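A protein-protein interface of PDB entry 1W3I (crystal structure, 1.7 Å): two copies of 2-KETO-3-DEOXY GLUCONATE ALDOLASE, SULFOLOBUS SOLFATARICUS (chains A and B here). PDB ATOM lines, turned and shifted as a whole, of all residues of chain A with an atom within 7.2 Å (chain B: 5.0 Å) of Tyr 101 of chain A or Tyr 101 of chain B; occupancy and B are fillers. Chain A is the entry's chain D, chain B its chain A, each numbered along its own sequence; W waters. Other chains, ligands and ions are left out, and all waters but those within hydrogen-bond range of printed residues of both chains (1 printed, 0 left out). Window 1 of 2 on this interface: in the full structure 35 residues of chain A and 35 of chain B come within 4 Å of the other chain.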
ATOM      1  N   GLY A  46      26.244  -2.510 -12.118  1.00  0.00           N
ATOM      2  CA  GLY A  46      25.424  -1.317 -12.096  1.00  0.00           C
ATOM      3  C   GLY A  46      25.883  -0.214 -11.113  1.00  0.00           C
ATOM      4  O   GLY A  46      25.902   0.963 -11.526  1.00  0.00           O
ATOM      5  N   PRO A  47      26.178  -0.522  -9.847  1.00  0.00           N
ATOM      6  CA  PRO A  47      26.613   0.515  -8.906  1.00  0.00           C
ATOM      7  C   PRO A  47      27.902   1.221  -9.336  1.00  0.00           C
ATOM      8  O   PRO A  47      28.176   2.315  -8.882  1.00  0.00           O
ATOM      9  CB  PRO A  47      26.768  -0.265  -7.572  1.00  0.00           C
ATOM     10  CG  PRO A  47      25.742  -1.332  -7.690  1.00  0.00           C
ATOM     11  CD  PRO A  47      25.901  -1.794  -9.146  1.00  0.00           C
ATOM     12  N   SER A  48      28.666   0.570 -10.201  1.00  0.00           N
ATOM     13  CA  SER A  48      29.914   1.134 -10.709  1.00  0.00           C
ATOM     14  C   SER A  48      29.735   2.031 -11.952  1.00  0.00           C
ATOM     15  O   SER A  48      30.691   2.653 -12.397  1.00  0.00           O
ATOM     16  CB  SER A  48      30.839  -0.022 -11.032  1.00  0.00           C
ATOM     17  OG  SER A  48      31.034  -0.829  -9.885  1.00  0.00           O
ATOM     18  N   LEU A  49      28.508   2.108 -12.474  1.00  0.00           N
ATOM     19  CA  LEU A  49      28.219   2.815 -13.714  1.00  0.00           C
ATOM     20  C   LEU A  49      27.618   4.174 -13.398  1.00  0.00           C
ATOM     21  O   LEU A  49      26.714   4.295 -12.542  1.00  0.00           O
ATOM     22  CB  LEU A  49      27.223   2.000 -14.562  1.00  0.00           C
ATOM     23  CG  LEU A  49      27.745   0.627 -14.995  1.00  0.00           C
ATOM     24  CD1 LEU A  49      26.675  -0.102 -15.791  1.00  0.00           C
ATOM     25  CD2 LEU A  49      29.059   0.785 -15.822  1.00  0.00           C
ATOM     26  N   LYS A  54      24.777   3.839 -17.555  1.00  0.00           N
ATOM     27  CA  LYS A  54      23.584   2.997 -17.427  1.00  0.00           C
ATOM     28  C   LYS A  54      22.729   3.096 -18.687  1.00  0.00           C
ATOM     29  O   LYS A  54      22.213   2.089 -19.177  1.00  0.00           O
ATOM     30  CB  LYS A  54      22.792   3.330 -16.167  1.00  0.00           C
ATOM     31  CG  LYS A  54      23.426   2.767 -14.905  1.00  0.00           C
ATOM     32  CD  LYS A  54      22.469   2.975 -13.707  1.00  0.00           C
ATOM     33  CE  LYS A  54      23.038   2.415 -12.387  1.00  0.00           C
ATOM     34  NZ  LYS A  54      24.139   3.225 -11.823  1.00  0.00           N
ATOM     35  N   GLN A  71      17.725  -1.458 -15.061  1.00  0.00           N
ATOM     36  CA  GLN A  71      17.931  -1.072 -13.643  1.00  0.00           C
ATOM     37  C   GLN A  71      18.507   0.348 -13.624  1.00  0.00           C
ATOM     38  O   GLN A  71      19.466   0.657 -14.362  1.00  0.00           O
ATOM     39  CB  GLN A  71      18.873  -2.110 -12.981  1.00  0.00           C
ATOM     40  CG  GLN A  71      18.804  -2.128 -11.447  1.00  0.00           C
ATOM     41  CD  GLN A  71      19.439  -0.892 -10.781  1.00  0.00           C
ATOM     42  OE1 GLN A  71      18.851  -0.316  -9.849  1.00  0.00           O
ATOM     43  NE2 GLN A  71      20.658  -0.505 -11.241  1.00  0.00           N
ATOM     44  N   GLY A  73      18.641   2.475 -10.479  1.00  0.00           N
ATOM     45  CA  GLY A  73      18.763   3.070  -9.150  1.00  0.00           C
ATOM     46  C   GLY A  73      20.118   3.629  -8.789  1.00  0.00           C
ATOM     47  O   GLY A  73      21.130   3.363  -9.431  1.00  0.00           O
ATOM     48  N   GLY A  74      20.135   4.427  -7.720  1.00  0.00           N
ATOM     49  CA  GLY A  74      21.408   4.865  -7.163  1.00  0.00           C
ATOM     50  C   GLY A  74      21.106   5.880  -6.085  1.00  0.00           C
ATOM     51  O   GLY A  74      19.963   5.965  -5.605  1.00  0.00           O
ATOM     52  N   LEU A  75      22.138   6.619  -5.681  1.00  0.00           N
ATOM     53  CA  LEU A  75      22.018   7.476  -4.498  1.00  0.00           C
ATOM     54  C   LEU A  75      21.741   8.937  -4.819  1.00  0.00           C
ATOM     55  O   LEU A  75      21.764   9.805  -3.928  1.00  0.00           O
ATOM     56  CB  LEU A  75      23.316   7.347  -3.682  1.00  0.00           C
ATOM     57  CG  LEU A  75      23.506   6.003  -3.001  1.00  0.00           C
ATOM     58  CD1 LEU A  75      24.895   6.102  -2.326  1.00  0.00           C
ATOM     59  CD2 LEU A  75      22.404   5.798  -1.929  1.00  0.00           C
ATOM     60  N   ASN A  76      21.499   9.210  -6.096  1.00  0.00           N
ATOM     61  CA  ASN A  76      21.038  10.521  -6.519  1.00  0.00           C
ATOM     62  C   ASN A  76      19.669  10.287  -7.172  1.00  0.00           C
ATOM     63  O   ASN A  76      19.585   9.805  -8.296  1.00  0.00           O
ATOM     64  CB  ASN A  76      22.014  11.102  -7.516  1.00  0.00           C
ATOM     65  CG  ASN A  76      21.637  12.490  -7.966  1.00  0.00           C
ATOM     66  OD1 ASN A  76      20.459  12.776  -8.189  1.00  0.00           O
ATOM     67  ND2 ASN A  76      22.633  13.363  -8.097  1.00  0.00           N
ATOM     68  N   TYR A  98      17.374  -1.404  -7.189  1.00  0.00           N
ATOM     69  CA  TYR A  98      17.686  -1.833  -5.835  1.00  0.00           C
ATOM     70  C   TYR A  98      17.428  -0.692  -4.870  1.00  0.00           C
ATOM     71  O   TYR A  98      17.173   0.467  -5.261  1.00  0.00           O
ATOM     72  CB  TYR A  98      19.163  -2.341  -5.679  1.00  0.00           C
ATOM     73  CG  TYR A  98      20.179  -1.640  -6.568  1.00  0.00           C
ATOM     74  CD1 TYR A  98      20.347  -0.248  -6.560  1.00  0.00           C
ATOM     75  CD2 TYR A  98      20.922  -2.391  -7.472  1.00  0.00           C
ATOM     76  CE1 TYR A  98      21.297   0.375  -7.457  1.00  0.00           C
ATOM     77  CE2 TYR A  98      21.870  -1.785  -8.325  1.00  0.00           C
ATOM     78  CZ  TYR A  98      22.025  -0.414  -8.305  1.00  0.00           C
ATOM     79  OH  TYR A  98      22.938   0.108  -9.192  1.00  0.00           O
ATOM     80  N   ALA A  99      17.428  -1.041  -3.591  1.00  0.00           N
ATOM     81  CA  ALA A  99      17.251  -0.013  -2.560  1.00  0.00           C
ATOM     82  C   ALA A  99      18.494   0.855  -2.482  1.00  0.00           C
ATOM     83  O   ALA A  99      19.561   0.401  -2.811  1.00  0.00           O
ATOM     84  CB  ALA A  99      16.986  -0.674  -1.198  1.00  0.00           C
ATOM     85  N   PRO A 100      18.355   2.105  -2.041  1.00  0.00           N
ATOM     86  CA  PRO A 100      19.516   2.987  -1.807  1.00  0.00           C
ATOM     87  C   PRO A 100      20.524   2.281  -0.931  1.00  0.00           C
ATOM     88  O   PRO A 100      20.159   1.756   0.133  1.00  0.00           O
ATOM     89  CB  PRO A 100      18.903   4.159  -1.030  1.00  0.00           C
ATOM     90  CG  PRO A 100      17.446   4.141  -1.437  1.00  0.00           C
ATOM     91  CD  PRO A 100      17.077   2.736  -1.670  1.00  0.00           C
ATOM     92  N   TYR A 101      21.758   2.156  -1.437  1.00  0.00           N
ATOM     93  CA  TYR A 101      22.773   1.367  -0.744  1.00  0.00           C
ATOM     94  C   TYR A 101      23.681   2.215   0.139  1.00  0.00           C
ATOM     95  O   TYR A 101      23.484   3.429   0.276  1.00  0.00           O
ATOM     96  CB  TYR A 101      23.603   0.540  -1.756  1.00  0.00           C
ATOM     97  CG  TYR A 101      23.999   1.298  -2.981  1.00  0.00           C
ATOM     98  CD1 TYR A 101      25.096   2.177  -2.975  1.00  0.00           C
ATOM     99  CD2 TYR A 101      23.307   1.138  -4.173  1.00  0.00           C
ATOM    100  CE1 TYR A 101      25.456   2.880  -4.142  1.00  0.00           C
ATOM    101  CE2 TYR A 101      23.680   1.806  -5.328  1.00  0.00           C
ATOM    102  CZ  TYR A 101      24.730   2.683  -5.313  1.00  0.00           C
ATOM    103  OH  TYR A 101      25.050   3.324  -6.506  1.00  0.00           O
ATOM    104  N   TYR A 102      24.638   1.536   0.767  1.00  0.00           N
ATOM    105  CA  TYR A 102      25.649   2.127   1.644  1.00  0.00           C
ATOM    106  C   TYR A 102      25.076   2.588   2.999  1.00  0.00           C
ATOM    107  O   TYR A 102      25.456   2.062   4.039  1.00  0.00           O
ATOM    108  CB  TYR A 102      26.471   3.236   0.914  1.00  0.00           C
ATOM    109  CG  TYR A 102      27.600   3.806   1.772  1.00  0.00           C
ATOM    110  CD1 TYR A 102      28.921   3.370   1.617  1.00  0.00           C
ATOM    111  CD2 TYR A 102      27.333   4.788   2.731  1.00  0.00           C
ATOM    112  CE1 TYR A 102      29.964   3.907   2.399  1.00  0.00           C
ATOM    113  CE2 TYR A 102      28.345   5.303   3.538  1.00  0.00           C
ATOM    114  CZ  TYR A 102      29.658   4.861   3.363  1.00  0.00           C
ATOM    115  OH  TYR A 102      30.691   5.362   4.155  1.00  0.00           O
ATOM    116  N   TYR A 103      24.161   3.552   3.002  1.00  0.00           N
ATOM    117  CA  TYR A 103      23.795   4.216   4.258  1.00  0.00           C
ATOM    118  C   TYR A 103      23.003   3.271   5.168  1.00  0.00           C
ATOM    119  O   TYR A 103      21.950   2.780   4.777  1.00  0.00           O
ATOM    120  CB  TYR A 103      22.963   5.479   3.987  1.00  0.00           C
ATOM    121  CG  TYR A 103      23.694   6.477   3.159  1.00  0.00           C
ATOM    122  CD1 TYR A 103      23.298   6.719   1.833  1.00  0.00           C
ATOM    123  CD2 TYR A 103      24.776   7.207   3.685  1.00  0.00           C
ATOM    124  CE1 TYR A 103      24.005   7.659   1.024  1.00  0.00           C
ATOM    125  CE2 TYR A 103      25.483   8.155   2.892  1.00  0.00           C
ATOM    126  CZ  TYR A 103      25.086   8.367   1.581  1.00  0.00           C
ATOM    127  OH  TYR A 103      25.773   9.238   0.790  1.00  0.00           O
ATOM    128  N   PRO A 104      23.523   2.957   6.357  1.00  0.00           N
ATOM    129  CA  PRO A 104      22.782   2.111   7.292  1.00  0.00           C
ATOM    130  C   PRO A 104      21.610   2.853   7.904  1.00  0.00           C
ATOM    131  O   PRO A 104      21.578   4.087   7.977  1.00  0.00           O
ATOM    132  CB  PRO A 104      23.815   1.843   8.401  1.00  0.00           C
ATOM    133  CG  PRO A 104      25.115   2.093   7.717  1.00  0.00           C
ATOM    134  CD  PRO A 104      24.858   3.302   6.873  1.00  0.00           C
ATOM    135  N   MET A 106      18.417   3.517   7.223  1.00  0.00           N
ATOM    136  CA  MET A 106      17.481   4.394   6.547  1.00  0.00           C
ATOM    137  C   MET A 106      16.094   4.049   7.035  1.00  0.00           C
ATOM    138  O   MET A 106      15.758   2.875   7.234  1.00  0.00           O
ATOM    139  CB  MET A 106      17.589   4.254   5.021  1.00  0.00           C
ATOM    140  CG  MET A 106      18.943   4.721   4.529  1.00  0.00           C
ATOM    141  SD  MET A 106      19.149   4.539   2.724  1.00  0.00           S
ATOM    142  CE  MET A 106      17.966   5.804   2.150  1.00  0.00           C
ATOM    143  N   LEU A 111      12.679   4.908   2.567  1.00  0.00           N
ATOM    144  CA  LEU A 111      12.829   3.846   1.545  1.00  0.00           C
ATOM    145  C   LEU A 111      11.546   3.748   0.720  1.00  0.00           C
ATOM    146  O   LEU A 111      11.584   3.632  -0.512  1.00  0.00           O
ATOM    147  CB  LEU A 111      13.103   2.482   2.204  1.00  0.00           C
ATOM    148  CG  LEU A 111      14.475   2.467   2.880  1.00  0.00           C
ATOM    149  CD1 LEU A 111      14.574   1.309   3.848  1.00  0.00           C
ATOM    150  CD2 LEU A 111      15.607   2.363   1.812  1.00  0.00           C
ATOM    151  N   ALA A 134      23.812  -6.767  -0.184  1.00  0.00           N
ATOM    152  CA  ALA A 134      24.518  -5.722  -0.901  1.00  0.00           C
ATOM    153  C   ALA A 134      24.084  -4.299  -0.461  1.00  0.00           C
ATOM    154  O   ALA A 134      24.908  -3.381  -0.418  1.00  0.00           O
ATOM    155  CB  ALA A 134      24.286  -5.878  -2.453  1.00  0.00           C
ATOM    156  N   THR A 135      22.787  -4.089  -0.188  1.00  0.00           N
ATOM    157  CA  THR A 135      22.302  -2.715   0.004  1.00  0.00           C
ATOM    158  C   THR A 135      22.190  -2.339   1.456  1.00  0.00           C
ATOM    159  O   THR A 135      22.150  -1.138   1.763  1.00  0.00           O
ATOM    160  CB  THR A 135      20.919  -2.505  -0.595  1.00  0.00           C
ATOM    161  OG1 THR A 135      19.991  -3.396   0.042  1.00  0.00           O
ATOM    162  CG2 THR A 135      20.945  -2.805  -2.141  1.00  0.00           C
ATOM    163  N   GLY A 136      22.164  -3.347   2.312  1.00  0.00           N
ATOM    164  CA  GLY A 136      22.111  -3.124   3.743  1.00  0.00           C
ATOM    165  C   GLY A 136      20.712  -2.945   4.256  1.00  0.00           C
ATOM    166  O   GLY A 136      20.515  -2.626   5.458  1.00  0.00           O
ATOM    167  N   LYS A 137      19.725  -3.133   3.399  1.00  0.00           N
ATOM    168  CA  LYS A 137      18.360  -3.147   3.912  1.00  0.00           C
ATOM    169  C   LYS A 137      17.461  -4.069   3.122  1.00  0.00           C
ATOM    170  O   LYS A 137      17.784  -4.505   2.008  1.00  0.00           O
ATOM    171  CB  LYS A 137      17.788  -1.729   4.043  1.00  0.00           C
ATOM    172  CG  LYS A 137      17.648  -0.995   2.712  1.00  0.00           C
ATOM    173  CD  LYS A 137      18.937  -0.309   2.244  1.00  0.00           C
ATOM    174  CE  LYS A 137      19.604   0.717   3.292  1.00  0.00           C
ATOM    175  NZ  LYS A 137      20.934   1.204   2.762  1.00  0.00           N
ATOM    176  N   PRO A 262      37.403  -1.378  -8.665  1.00  0.00           N
ATOM    177  CA  PRO A 262      38.025  -2.460  -7.890  1.00  0.00           C
ATOM    178  C   PRO A 262      37.487  -3.884  -8.053  1.00  0.00           C
ATOM    179  O   PRO A 262      37.836  -4.758  -7.266  1.00  0.00           O
ATOM    180  CB  PRO A 262      37.817  -1.983  -6.440  1.00  0.00           C
ATOM    181  CG  PRO A 262      36.449  -1.276  -6.515  1.00  0.00           C
ATOM    182  CD  PRO A 262      36.485  -0.548  -7.865  1.00  0.00           C
ATOM    183  N   ILE A 263      36.628  -4.128  -9.043  1.00  0.00           N
ATOM    184  CA  ILE A 263      36.370  -5.504  -9.457  1.00  0.00           C
ATOM    185  C   ILE A 263      37.496  -5.845 -10.438  1.00  0.00           C
ATOM    186  O   ILE A 263      37.414  -5.521 -11.623  1.00  0.00           O
ATOM    187  CB  ILE A 263      34.974  -5.695 -10.112  1.00  0.00           C
ATOM    188  CG1 ILE A 263      33.837  -5.178  -9.192  1.00  0.00           C
ATOM    189  CG2 ILE A 263      34.764  -7.181 -10.439  1.00  0.00           C
ATOM    190  CD1 ILE A 263      33.713  -5.871  -7.771  1.00  0.00           C
ATOM    191  N   PRO B  47      29.158   9.045  -0.681  1.00  0.00           N
ATOM    192  CA  PRO B  47      28.712   8.082  -1.706  1.00  0.00           C
ATOM    193  C   PRO B  47      27.656   8.644  -2.649  1.00  0.00           C
ATOM    194  O   PRO B  47      27.535   8.092  -3.758  1.00  0.00           O
ATOM    195  CB  PRO B  47      28.194   6.912  -0.871  1.00  0.00           C
ATOM    196  CG  PRO B  47      29.056   6.977   0.389  1.00  0.00           C
ATOM    197  CD  PRO B  47      29.055   8.464   0.682  1.00  0.00           C
ATOM    198  N   GLY B  73      37.145   7.934  -2.153  1.00  0.00           N
ATOM    199  CA  GLY B  73      36.850   6.599  -2.638  1.00  0.00           C
ATOM    200  C   GLY B  73      35.563   6.418  -3.416  1.00  0.00           C
ATOM    201  O   GLY B  73      34.658   7.252  -3.397  1.00  0.00           O
ATOM    202  N   GLY B  74      35.492   5.284  -4.112  1.00  0.00           N
ATOM    203  CA  GLY B  74      34.268   4.894  -4.787  1.00  0.00           C
ATOM    204  C   GLY B  74      34.449   3.633  -5.589  1.00  0.00           C
ATOM    205  O   GLY B  74      35.435   2.925  -5.421  1.00  0.00           O
ATOM    206  N   LEU B  75      33.469   3.364  -6.441  1.00  0.00           N
ATOM    207  CA  LEU B  75      33.435   2.128  -7.224  1.00  0.00           C
ATOM    208  C   LEU B  75      34.030   2.288  -8.610  1.00  0.00           C
ATOM    209  O   LEU B  75      34.037   1.336  -9.415  1.00  0.00           O
ATOM    210  CB  LEU B  75      32.016   1.586  -7.256  1.00  0.00           C
ATOM    211  CG  LEU B  75      31.471   1.178  -5.888  1.00  0.00           C
ATOM    212  CD1 LEU B  75      30.056   0.656  -6.140  1.00  0.00           C
ATOM    213  CD2 LEU B  75      32.319   0.112  -5.267  1.00  0.00           C
ATOM    214  N   TYR B  98      36.973   5.047   2.139  1.00  0.00           N
ATOM    215  CA  TYR B  98      36.328   3.813   2.580  1.00  0.00           C
ATOM    216  C   TYR B  98      36.624   2.681   1.621  1.00  0.00           C
ATOM    217  O   TYR B  98      37.130   2.893   0.490  1.00  0.00           O
ATOM    218  CB  TYR B  98      34.800   3.965   2.778  1.00  0.00           C
ATOM    219  CG  TYR B  98      34.124   4.959   1.859  1.00  0.00           C
ATOM    220  CD1 TYR B  98      34.220   4.844   0.472  1.00  0.00           C
ATOM    221  CD2 TYR B  98      33.379   6.023   2.382  1.00  0.00           C
ATOM    222  CE1 TYR B  98      33.589   5.783  -0.374  1.00  0.00           C
ATOM    223  CE2 TYR B  98      32.746   6.960   1.551  1.00  0.00           C
ATOM    224  CZ  TYR B  98      32.858   6.844   0.182  1.00  0.00           C
ATOM    225  OH  TYR B  98      32.247   7.785  -0.636  1.00  0.00           O
ATOM    226  N   ALA B  99      36.274   1.471   2.050  1.00  0.00           N
ATOM    227  CA  ALA B  99      36.436   0.292   1.214  1.00  0.00           C
ATOM    228  C   ALA B  99      35.382   0.332   0.131  1.00  0.00           C
ATOM    229  O   ALA B  99      34.335   0.967   0.323  1.00  0.00           O
ATOM    230  CB  ALA B  99      36.268  -0.983   2.051  1.00  0.00           C
ATOM    231  N   PRO B 100      35.640  -0.342  -0.998  1.00  0.00           N
ATOM    232  CA  PRO B 100      34.615  -0.488  -2.043  1.00  0.00           C
ATOM    233  C   PRO B 100      33.331  -1.057  -1.471  1.00  0.00           C
ATOM    234  O   PRO B 100      33.377  -2.100  -0.800  1.00  0.00           O
ATOM    235  CB  PRO B 100      35.255  -1.481  -3.030  1.00  0.00           C
ATOM    236  CG  PRO B 100      36.749  -1.173  -2.889  1.00  0.00           C
ATOM    237  CD  PRO B 100      36.922  -0.989  -1.363  1.00  0.00           C
ATOM    238  N   TYR B 101      32.217  -0.358  -1.687  1.00  0.00           N
ATOM    239  CA  TYR B 101      30.953  -0.754  -1.020  1.00  0.00           C
ATOM    240  C   TYR B 101      30.049  -1.544  -1.972  1.00  0.00           C
ATOM    241  O   TYR B 101      30.451  -1.834  -3.112  1.00  0.00           O
ATOM    242  CB  TYR B 101      30.219   0.500  -0.458  1.00  0.00           C
ATOM    243  CG  TYR B 101      30.223   1.688  -1.410  1.00  0.00           C
ATOM    244  CD1 TYR B 101      29.305   1.775  -2.474  1.00  0.00           C
ATOM    245  CD2 TYR B 101      31.150   2.726  -1.242  1.00  0.00           C
ATOM    246  CE1 TYR B 101      29.336   2.895  -3.370  1.00  0.00           C
ATOM    247  CE2 TYR B 101      31.169   3.818  -2.080  1.00  0.00           C
ATOM    248  CZ  TYR B 101      30.279   3.897  -3.147  1.00  0.00           C
ATOM    249  OH  TYR B 101      30.342   5.016  -3.941  1.00  0.00           O
ATOM    250  N   TYR B 102      28.855  -1.883  -1.480  1.00  0.00           N
ATOM    251  CA  TYR B 102      27.852  -2.657  -2.244  1.00  0.00           C
ATOM    252  C   TYR B 102      28.232  -4.112  -2.479  1.00  0.00           C
ATOM    253  O   TYR B 102      27.610  -5.011  -1.914  1.00  0.00           O
ATOM    254  CB  TYR B 102      27.407  -1.930  -3.526  1.00  0.00           C
ATOM    255  CG  TYR B 102      26.272  -2.652  -4.224  1.00  0.00           C
ATOM    256  CD1 TYR B 102      24.972  -2.207  -4.096  1.00  0.00           C
ATOM    257  CD2 TYR B 102      26.519  -3.755  -5.046  1.00  0.00           C
ATOM    258  CE1 TYR B 102      23.925  -2.846  -4.725  1.00  0.00           C
ATOM    259  CE2 TYR B 102      25.489  -4.399  -5.690  1.00  0.00           C
ATOM    260  CZ  TYR B 102      24.191  -3.931  -5.541  1.00  0.00           C
ATOM    261  OH  TYR B 102      23.172  -4.564  -6.165  1.00  0.00           O
ATOM    262  N   TYR B 103      29.284  -4.374  -3.257  1.00  0.00           N
ATOM    263  CA  TYR B 103      29.539  -5.743  -3.708  1.00  0.00           C
ATOM    264  C   TYR B 103      29.959  -6.647  -2.541  1.00  0.00           C
ATOM    265  O   TYR B 103      30.978  -6.411  -1.917  1.00  0.00           O
ATOM    266  CB  TYR B 103      30.628  -5.733  -4.789  1.00  0.00           C
ATOM    267  CG  TYR B 103      30.233  -4.895  -5.986  1.00  0.00           C
ATOM    268  CD1 TYR B 103      30.939  -3.722  -6.293  1.00  0.00           C
ATOM    269  CD2 TYR B 103      29.195  -5.315  -6.859  1.00  0.00           C
ATOM    270  CE1 TYR B 103      30.566  -2.935  -7.399  1.00  0.00           C
ATOM    271  CE2 TYR B 103      28.826  -4.544  -7.971  1.00  0.00           C
ATOM    272  CZ  TYR B 103      29.535  -3.371  -8.230  1.00  0.00           C
ATOM    273  OH  TYR B 103      29.186  -2.581  -9.281  1.00  0.00           O
ATOM    274  N   ALA B 134      28.425  -0.158   6.695  1.00  0.00           N
ATOM    275  CA  ALA B 134      28.099   0.586   5.497  1.00  0.00           C
ATOM    276  C   ALA B 134      28.663  -0.087   4.253  1.00  0.00           C
ATOM    277  O   ALA B 134      27.986  -0.135   3.207  1.00  0.00           O
ATOM    278  CB  ALA B 134      28.579   2.051   5.600  1.00  0.00           C
ATOM    279  N   THR B 135      29.883  -0.612   4.338  1.00  0.00           N
ATOM    280  CA  THR B 135      30.581  -1.048   3.117  1.00  0.00           C
ATOM    281  C   THR B 135      30.473  -2.527   2.896  1.00  0.00           C
ATOM    282  O   THR B 135      30.730  -3.008   1.791  1.00  0.00           O
ATOM    283  CB  THR B 135      32.106  -0.693   3.118  1.00  0.00           C
ATOM    284  OG1 THR B 135      32.751  -1.319   4.246  1.00  0.00           O
ATOM    285  CG2 THR B 135      32.302   0.811   3.327  1.00  0.00           C
ATOM    286  N   LYS B 137      32.468  -4.569   4.339  1.00  0.00           N
ATOM    287  CA  LYS B 137      33.738  -5.242   4.618  1.00  0.00           C
ATOM    288  C   LYS B 137      34.547  -4.617   5.689  1.00  0.00           C
ATOM    289  O   LYS B 137      34.291  -3.492   6.099  1.00  0.00           O
ATOM    290  CB  LYS B 137      34.548  -5.545   3.371  1.00  0.00           C
ATOM    291  CG  LYS B 137      34.829  -4.392   2.483  1.00  0.00           C
ATOM    292  CD  LYS B 137      33.712  -4.088   1.512  1.00  0.00           C
ATOM    293  CE  LYS B 137      33.267  -5.196   0.458  1.00  0.00           C
ATOM    294  NZ  LYS B 137      32.043  -4.544  -0.124  1.00  0.00           N
HETATM  295  O   HOH W   1      33.665  -1.304  -9.758  1.00  0.00           O
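The side-chain hydroxyl of Tyr 103 of chain B sits at hydrogen-bond distance from the side-chain hydroxyl of Ser 48 of chain A, 2.6 Å away. The backbone carbonyl oxygen of Tyr 102 of chain A lies close to the backbone carbonyl oxygen of Ala 134 of chain B, at 3.5 Å. The backbone carbonyl oxygen (O) of Tyr 102 of chain B lies close to the backbone carbonyl oxygen (O) of Ala 134 of chain A (3.5 Å).
O of Pro 100 of chain B is in hydrogen-bond range of NZ of Lys 137 of chain B (2.9 Å). The backbone carbonyl oxygen (O) of Tyr 103 of chain B sits at hydrogen-bond distance from the side-chain amino group (NZ) of Lys 137 of chain B. O of Thr 135 of chain B is in hydrogen-bond range of NZ of Lys 137 of chain B (2.8 Å). The side-chain hydroxyl (OH) of Tyr 98 of chain A sits at hydrogen-bond distance from the side-chain amide nitrogen (NE2) of Gln 71 of chain A (3.1 Å). O of Tyr 103 of chain A is in hydrogen-bond range of NZ of Lys 137 of chain A (2.8 Å). O of Thr 135 of chain A is in hydrogen-bond range of NZ of Lys 137 of chain A, 2.8 Å away.
Among the printed residues, pairs that only touch across the chains: Tyr 102 of chain A with Tyr 98 of chain B, Tyr 103 of chain A with Pro 47 of chain B, Pro 47 of chain A with Tyr 103 of chain B, Tyr 98 of chain A with Tyr 102 of chain B, Pro 262 of chain A with Leu 75 of chain B, Leu 75 of chain A with Pro 47 of chain B, Tyr 102 of chain A with Pro 47 of chain B, Pro 262 of chain A with Pro 100 of chain B, Pro 47 of chain A with Tyr 102 of chain B, Tyr 102 of chain A with Tyr 101 of chain B, Ser 48 of chain A with Leu 75 of chain B, Pro 47 of chain A with Leu 75 of chain B, Tyr 101 of chain A with Tyr 102 of chain B, Ile 263 of chain A with Tyr 103 of chain B, Thr 135 of chain A with Tyr 102 of chain B, Tyr 101 of chain A with Tyr 101 of chain B and Tyr 102 of chain A with Thr 135 of chain B.
Gln 71 of chain A touches none of the printed residues of chain B. Tyr 101 of chain A touches just these residues of chain B: Tyr 101 and Tyr 102. Printed residues of chain B within 4 Å of Ala 134 of chain A: Tyr 102. Of the printed residues of chain A, Pro 47 of chain B touches Leu 75, Tyr 102 and Tyr 103. Gly 74 of chain B touches none of the printed residues of chain A. The nearest printed residue of chain B that does not touch Tyr 101 of chain A is Leu 75 of chain B (5.5 Å). The nearest residue of chain A that does not touch Tyr 101 of chain B is Leu 75 of chain A (5.6 Å).
Of the 25 printed residues of chain A, 11 touch a printed residue of chain B. Printed residues of chain A that touch a printed residue of chain B: Pro 47, Ser 48, Leu 75, Tyr 98, Tyr 101, Tyr 102, Tyr 103, Ala 134, Thr 135, Pro 262 and Ile 263. Of the 13 printed residues of chain B, 9 touch a printed residue of chain A. Among the printed residues, 20 pairs touch across the chains. Among the printed residues, no Asp or Glu carboxylate lies within 4 Å of a Lys or Arg side-chain nitrogen of the other chain.
Pro 47 of chain A touches Tyr 102 of chain B, and with the chains exchanged Tyr 102 of chain A touches Pro 47 of chain B. Tyr 98 of chain A touches Tyr 102 of chain B, and with the chains exchanged Tyr 102 of chain A touches Tyr 98 of chain B. Tyr 101 of chain A touches its own counterpart, Tyr 101 of chain B. Tyr 102 of chain A touches Thr 135 of chain B, and with the chains exchanged Thr 135 of chain A touches Tyr 102 of chain B. Of the 20 pairs that touch across the chains among the printed residues, 15 have their exchanged pair printed and touching as well.
Water W1 bridges OG of Ser 48 of chain A (2.7 Å) and O of Leu 75 of chain B (2.7 Å).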
